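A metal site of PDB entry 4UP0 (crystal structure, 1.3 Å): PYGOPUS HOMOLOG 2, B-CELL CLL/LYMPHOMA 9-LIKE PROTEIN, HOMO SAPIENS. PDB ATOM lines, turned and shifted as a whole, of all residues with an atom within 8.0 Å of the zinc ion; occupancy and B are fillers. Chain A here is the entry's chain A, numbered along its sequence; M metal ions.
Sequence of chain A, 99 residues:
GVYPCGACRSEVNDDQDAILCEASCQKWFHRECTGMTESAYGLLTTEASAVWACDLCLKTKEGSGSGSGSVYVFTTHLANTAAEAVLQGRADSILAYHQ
Four residues have an atom within 4 Å of the zinc ion: Cys 5, Cys 8, His 30 and Cys 33. The nearest printed residue that does not touch the zinc ion is Ala 7 (4.8 Å).
ND1 of His 30 is bound to the zinc ion (2.1 Å). SG of Cys 33 binds the zinc ion, at 2.3 Å. The side-chain sulfur (SG) of Cys 8 binds the zinc ion. The side-chain sulfur (SG) of Cys 5 is bound to the zinc ion, 2.3 Å away. The zinc ion has four donor atoms within binding distance.
The backbone carbonyl oxygen of Glu 11 sits at hydrogen-bond distance from a ring nitrogen (NE2) of His 30. A ring nitrogen (NE2) of His 30 sits at hydrogen-bond distance from the side-chain amide oxygen of Gln 16, at 2.9 Å. The side-chain sulfur of Cys 8 lies close to the backbone NH of Ser 10 (3.5 Å). The side-chain sulfur of Cys 5 lies close to the backbone NH of Ala 7 (3.4 Å). The backbone NH (N) of Cys 5 sits at hydrogen-bond distance from the backbone carbonyl oxygen (O) of Ser 10 (2.8 Å).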
ATOM      1  N   PRO A   4      20.634  -4.160  -9.433  1.00  0.00           N
ATOM      2  CA  PRO A   4      21.687  -5.117  -9.290  1.00  0.00           C
ATOM      3  C   PRO A   4      22.159  -5.696 -10.656  1.00  0.00           C
ATOM      4  O   PRO A   4      21.350  -5.774 -11.573  1.00  0.00           O
ATOM      5  CB  PRO A   4      21.045  -6.226  -8.504  1.00  0.00           C
ATOM      6  CG  PRO A   4      19.632  -6.206  -8.933  1.00  0.00           C
ATOM      7  CD  PRO A   4      19.290  -4.772  -9.315  1.00  0.00           C
ATOM      8  N   CYS A   5      23.406  -6.060 -10.741  1.00  0.00           N
ATOM      9  CA  CYS A   5      23.946  -6.583 -11.973  1.00  0.00           C
ATOM     10  C   CYS A   5      23.323  -7.940 -12.249  1.00  0.00           C
ATOM     11  O   CYS A   5      23.223  -8.835 -11.405  1.00  0.00           O
ATOM     12  CB  CYS A   5      25.466  -6.763 -11.745  1.00  0.00           C
ATOM     13  SG  CYS A   5      26.328  -7.555 -13.149  1.00  0.00           S
ATOM     14  N   GLY A   6      22.917  -8.100 -13.515  1.00  0.00           N
ATOM     15  CA  GLY A   6      22.249  -9.351 -13.911  1.00  0.00           C
ATOM     16  C   GLY A   6      23.164 -10.588 -13.848  1.00  0.00           C
ATOM     17  O   GLY A   6      22.682 -11.717 -13.813  1.00  0.00           O
ATOM     18  N   ALA A   7      24.496 -10.376 -13.793  1.00  0.00           N
ATOM     19  CA  ALA A   7      25.454 -11.473 -13.683  1.00  0.00           C
ATOM     20  C   ALA A   7      25.917 -11.705 -12.251  1.00  0.00           C
ATOM     21  O   ALA A   7      25.745 -12.785 -11.741  1.00  0.00           O
ATOM     22  CB  ALA A   7      26.631 -11.180 -14.613  1.00  0.00           C
ATOM     23  N   CYS A   8      26.476 -10.688 -11.577  1.00  0.00           N
ATOM     24  CA  CYS A   8      27.039 -10.936 -10.257  1.00  0.00           C
ATOM     25  C   CYS A   8      26.086 -10.603  -9.144  1.00  0.00           C
ATOM     26  O   CYS A   8      26.394 -10.945  -8.003  1.00  0.00           O
ATOM     27  CB  CYS A   8      28.336 -10.112 -10.068  1.00  0.00           C
ATOM     28  SG  CYS A   8      28.078  -8.311  -9.870  1.00  0.00           S
ATOM     29  N   ARG A   9      24.929  -9.994  -9.476  1.00  0.00           N
ATOM     30  CA  ARG A   9      23.864  -9.641  -8.540  1.00  0.00           C
ATOM     31  C   ARG A   9      24.251  -8.580  -7.536  1.00  0.00           C
ATOM     32  O   ARG A   9      23.470  -8.303  -6.650  1.00  0.00           O
ATOM     33  CB  ARG A   9      23.321 -10.928  -7.772  1.00  0.00           C
ATOM     34  CG  ARG A   9      22.734 -11.996  -8.761  1.00  0.00           C
ATOM     35  CD  ARG A   9      21.598 -11.464  -9.647  1.00  0.00           C
ATOM     36  NE  ARG A   9      20.854 -12.582 -10.240  1.00  0.00           N
ATOM     37  CZ  ARG A   9      19.958 -12.494 -11.209  1.00  0.00           C
ATOM     38  NH1 ARG A   9      19.697 -11.346 -11.842  1.00  0.00           N
ATOM     39  NH2 ARG A   9      19.336 -13.649 -11.565  1.00  0.00           N
ATOM     40  N   SER A  10      25.424  -7.922  -7.641  1.00  0.00           N
ATOM     41  CA  SER A  10      25.777  -6.782  -6.789  1.00  0.00           C
ATOM     42  C   SER A  10      25.310  -5.494  -7.426  1.00  0.00           C
ATOM     43  O   SER A  10      25.144  -5.417  -8.634  1.00  0.00           O
ATOM     44  CB  SER A  10      27.286  -6.723  -6.467  1.00  0.00           C
ATOM     45  OG  SER A  10      27.607  -7.848  -5.724  1.00  0.00           O
ATOM     46  N   GLU A  11      25.236  -4.427  -6.599  1.00  0.00           N
ATOM     47  CA  GLU A  11      24.731  -3.179  -7.093  1.00  0.00           C
ATOM     48  C   GLU A  11      25.577  -2.664  -8.309  1.00  0.00           C
ATOM     49  O   GLU A  11      26.780  -2.706  -8.352  1.00  0.00           O
ATOM     50  CB  GLU A  11      24.646  -2.090  -5.982  1.00  0.00           C
ATOM     51  CG  GLU A  11      25.896  -1.570  -5.516  1.00  0.00           C
ATOM     52  CD  GLU A  11      25.703  -0.296  -4.626  1.00  0.00           C
ATOM     53  OE1 GLU A  11      24.539   0.252  -4.379  1.00  0.00           O
ATOM     54  OE2 GLU A  11      26.749   0.079  -4.120  1.00  0.00           O
ATOM     55  N   VAL A  12      24.856  -2.014  -9.235  1.00  0.00           N
ATOM     56  CA  VAL A  12      25.473  -1.278 -10.327  1.00  0.00           C
ATOM     57  C   VAL A  12      25.351   0.195  -9.983  1.00  0.00           C
ATOM     58  O   VAL A  12      24.238   0.708  -9.823  1.00  0.00           O
ATOM     59  CB  VAL A  12      24.701  -1.539 -11.664  1.00  0.00           C
ATOM     60  CG1 VAL A  12      25.305  -0.750 -12.816  1.00  0.00           C
ATOM     61  CG2 VAL A  12      24.764  -3.030 -11.970  1.00  0.00           C
ATOM     62  N   GLN A  16      30.201   3.189 -12.529  1.00  0.00           N
ATOM     63  CA  GLN A  16      30.813   1.963 -13.095  1.00  0.00           C
ATOM     64  C   GLN A  16      30.436   1.824 -14.567  1.00  0.00           C
ATOM     65  O   GLN A  16      29.375   2.262 -14.996  1.00  0.00           O
ATOM     66  CB  GLN A  16      30.215   0.776 -12.316  1.00  0.00           C
ATOM     67  CG  GLN A  16      30.650   0.758 -10.845  1.00  0.00           C
ATOM     68  CD  GLN A  16      30.040  -0.390 -10.088  1.00  0.00           C
ATOM     69  OE1 GLN A  16      28.861  -0.672 -10.173  1.00  0.00           O
ATOM     70  NE2 GLN A  16      30.902  -1.082  -9.390  1.00  0.00           N
ATOM     71  N   ASP A  17      31.292   1.207 -15.363  1.00  0.00           N
ATOM     72  CA  ASP A  17      30.875   0.831 -16.706  1.00  0.00           C
ATOM     73  C   ASP A  17      29.800  -0.236 -16.620  1.00  0.00           C
ATOM     74  O   ASP A  17      30.016  -1.283 -15.977  1.00  0.00           O
ATOM     75  CB  ASP A  17      32.048   0.263 -17.502  1.00  0.00           C
ATOM     76  CG  ASP A  17      33.146   1.253 -17.861  1.00  0.00           C
ATOM     77  OD1 ASP A  17      32.996   2.436 -17.644  1.00  0.00           O
ATOM     78  OD2 ASP A  17      34.129   0.729 -18.451  1.00  0.00           O
ATOM     79  N   ALA A  18      28.658  -0.025 -17.290  1.00  0.00           N
ATOM     80  CA  ALA A  18      27.569  -0.989 -17.230  1.00  0.00           C
ATOM     81  C   ALA A  18      26.697  -0.782 -18.422  1.00  0.00           C
ATOM     82  O   ALA A  18      26.566   0.369 -18.946  1.00  0.00           O
ATOM     83  CB  ALA A  18      26.807  -0.902 -15.928  1.00  0.00           C
ATOM     84  N   TRP A  28      20.588  -4.333 -15.991  1.00  0.00           N
ATOM     85  CA  TRP A  28      21.915  -3.774 -16.120  1.00  0.00           C
ATOM     86  C   TRP A  28      22.991  -4.809 -15.776  1.00  0.00           C
ATOM     87  O   TRP A  28      22.777  -5.599 -14.844  1.00  0.00           O
ATOM     88  CB  TRP A  28      22.076  -2.586 -15.155  1.00  0.00           C
ATOM     89  CG  TRP A  28      21.343  -1.375 -15.643  1.00  0.00           C
ATOM     90  CD1 TRP A  28      20.035  -0.965 -15.330  1.00  0.00           C
ATOM     91  CD2 TRP A  28      21.830  -0.407 -16.570  1.00  0.00           C
ATOM     92  NE1 TRP A  28      19.753   0.197 -16.037  1.00  0.00           N
ATOM     93  CE2 TRP A  28      20.817   0.548 -16.813  1.00  0.00           C
ATOM     94  CE3 TRP A  28      23.064  -0.272 -17.234  1.00  0.00           C
ATOM     95  CZ2 TRP A  28      21.010   1.617 -17.673  1.00  0.00           C
ATOM     96  CZ3 TRP A  28      23.247   0.790 -18.086  1.00  0.00           C
ATOM     97  CH2 TRP A  28      22.224   1.753 -18.287  1.00  0.00           C
ATOM     98  N   PHE A  29      24.118  -4.747 -16.499  1.00  0.00           N
ATOM     99  CA  PHE A  29      25.247  -5.614 -16.236  1.00  0.00           C
ATOM    100  C   PHE A  29      26.523  -4.797 -16.160  1.00  0.00           C
ATOM    101  O   PHE A  29      26.788  -4.005 -17.056  1.00  0.00           O
ATOM    102  CB  PHE A  29      25.417  -6.601 -17.400  1.00  0.00           C
ATOM    103  CG  PHE A  29      24.373  -7.697 -17.446  1.00  0.00           C
ATOM    104  CD1 PHE A  29      23.039  -7.422 -17.833  1.00  0.00           C
ATOM    105  CD2 PHE A  29      24.730  -8.999 -17.094  1.00  0.00           C
ATOM    106  CE1 PHE A  29      22.113  -8.466 -17.895  1.00  0.00           C
ATOM    107  CE2 PHE A  29      23.785 -10.055 -17.138  1.00  0.00           C
ATOM    108  CZ  PHE A  29      22.500  -9.756 -17.487  1.00  0.00           C
ATOM    109  N   HIS A  30      27.356  -5.016 -15.146  1.00  0.00           N
ATOM    110  CA  HIS A  30      28.681  -4.412 -15.147  1.00  0.00           C
ATOM    111  C   HIS A  30      29.399  -4.888 -16.437  1.00  0.00           C
ATOM    112  O   HIS A  30      29.368  -6.044 -16.738  1.00  0.00           O
ATOM    113  CB  HIS A  30      29.543  -4.861 -13.976  1.00  0.00           C
ATOM    114  CG  HIS A  30      29.010  -4.490 -12.630  1.00  0.00           C
ATOM    115  ND1 HIS A  30      28.581  -5.428 -11.709  1.00  0.00           N
ATOM    116  CD2 HIS A  30      28.909  -3.278 -12.031  1.00  0.00           C
ATOM    117  CE1 HIS A  30      28.197  -4.810 -10.587  1.00  0.00           C
ATOM    118  NE2 HIS A  30      28.410  -3.493 -10.752  1.00  0.00           N
ATOM    119  N   ARG A  31      30.088  -3.946 -17.084  1.00  0.00           N
ATOM    120  CA  ARG A  31      30.902  -4.295 -18.252  1.00  0.00           C
ATOM    121  C   ARG A  31      31.813  -5.461 -17.922  1.00  0.00           C
ATOM    122  O   ARG A  31      31.924  -6.453 -18.698  1.00  0.00           O
ATOM    123  CB  ARG A  31      31.690  -3.097 -18.737  1.00  0.00           C
ATOM    124  CG  ARG A  31      32.491  -3.410 -20.027  1.00  0.00           C
ATOM    125  CD  ARG A  31      33.443  -2.281 -20.333  1.00  0.00           C
ATOM    126  NE  ARG A  31      34.475  -2.027 -19.338  1.00  0.00           N
ATOM    127  CZ  ARG A  31      35.587  -2.732 -19.205  1.00  0.00           C
ATOM    128  NH1 ARG A  31      35.841  -3.789 -20.018  1.00  0.00           N
ATOM    129  NH2 ARG A  31      36.513  -2.356 -18.340  1.00  0.00           N
ATOM    130  N   GLU A  32      32.532  -5.365 -16.807  1.00  0.00           N
ATOM    131  CA  GLU A  32      33.537  -6.375 -16.468  1.00  0.00           C
ATOM    132  C   GLU A  32      32.894  -7.699 -16.075  1.00  0.00           C
ATOM    133  O   GLU A  32      33.588  -8.710 -16.104  1.00  0.00           O
ATOM    134  CB  GLU A  32      34.427  -5.828 -15.362  1.00  0.00           C
ATOM    135  CG  GLU A  32      35.237  -4.668 -15.825  1.00  0.00           C
ATOM    136  CD  GLU A  32      36.329  -4.187 -14.856  1.00  0.00           C
ATOM    137  OE1 GLU A  32      37.226  -5.007 -14.516  1.00  0.00           O
ATOM    138  OE2 GLU A  32      36.349  -2.996 -14.482  1.00  0.00           O
ATOM    139  N   CYS A  33      31.618  -7.808 -15.854  1.00  0.00           N
ATOM    140  CA  CYS A  33      30.962  -9.079 -15.607  1.00  0.00           C
ATOM    141  C   CYS A  33      30.520  -9.785 -16.861  1.00  0.00           C
ATOM    142  O   CYS A  33      29.977 -10.897 -16.836  1.00  0.00           O
ATOM    143  CB  CYS A  33      29.735  -8.879 -14.687  1.00  0.00           C
ATOM    144  SG  CYS A  33      30.219  -8.430 -12.990  1.00  0.00           S
ATOM    145  N   THR A  34      30.710  -9.153 -17.987  1.00  0.00           N
ATOM    146  CA  THR A  34      30.240  -9.685 -19.266  1.00  0.00           C
ATOM    147  C   THR A  34      31.409 -10.145 -20.183  1.00  0.00           C
ATOM    148  O   THR A  34      31.134 -10.777 -21.184  1.00  0.00           O
ATOM    149  CB  THR A  34      29.453  -8.649 -20.069  1.00  0.00           C
ATOM    150  OG1 THR A  34      30.308  -7.595 -20.534  1.00  0.00           O
ATOM    151  CG2 THR A  34      28.290  -8.078 -19.259  1.00  0.00           C
HETATM  152 ZN    ZN M   1      28.369  -7.483 -12.008  1.00  0.00          ZN
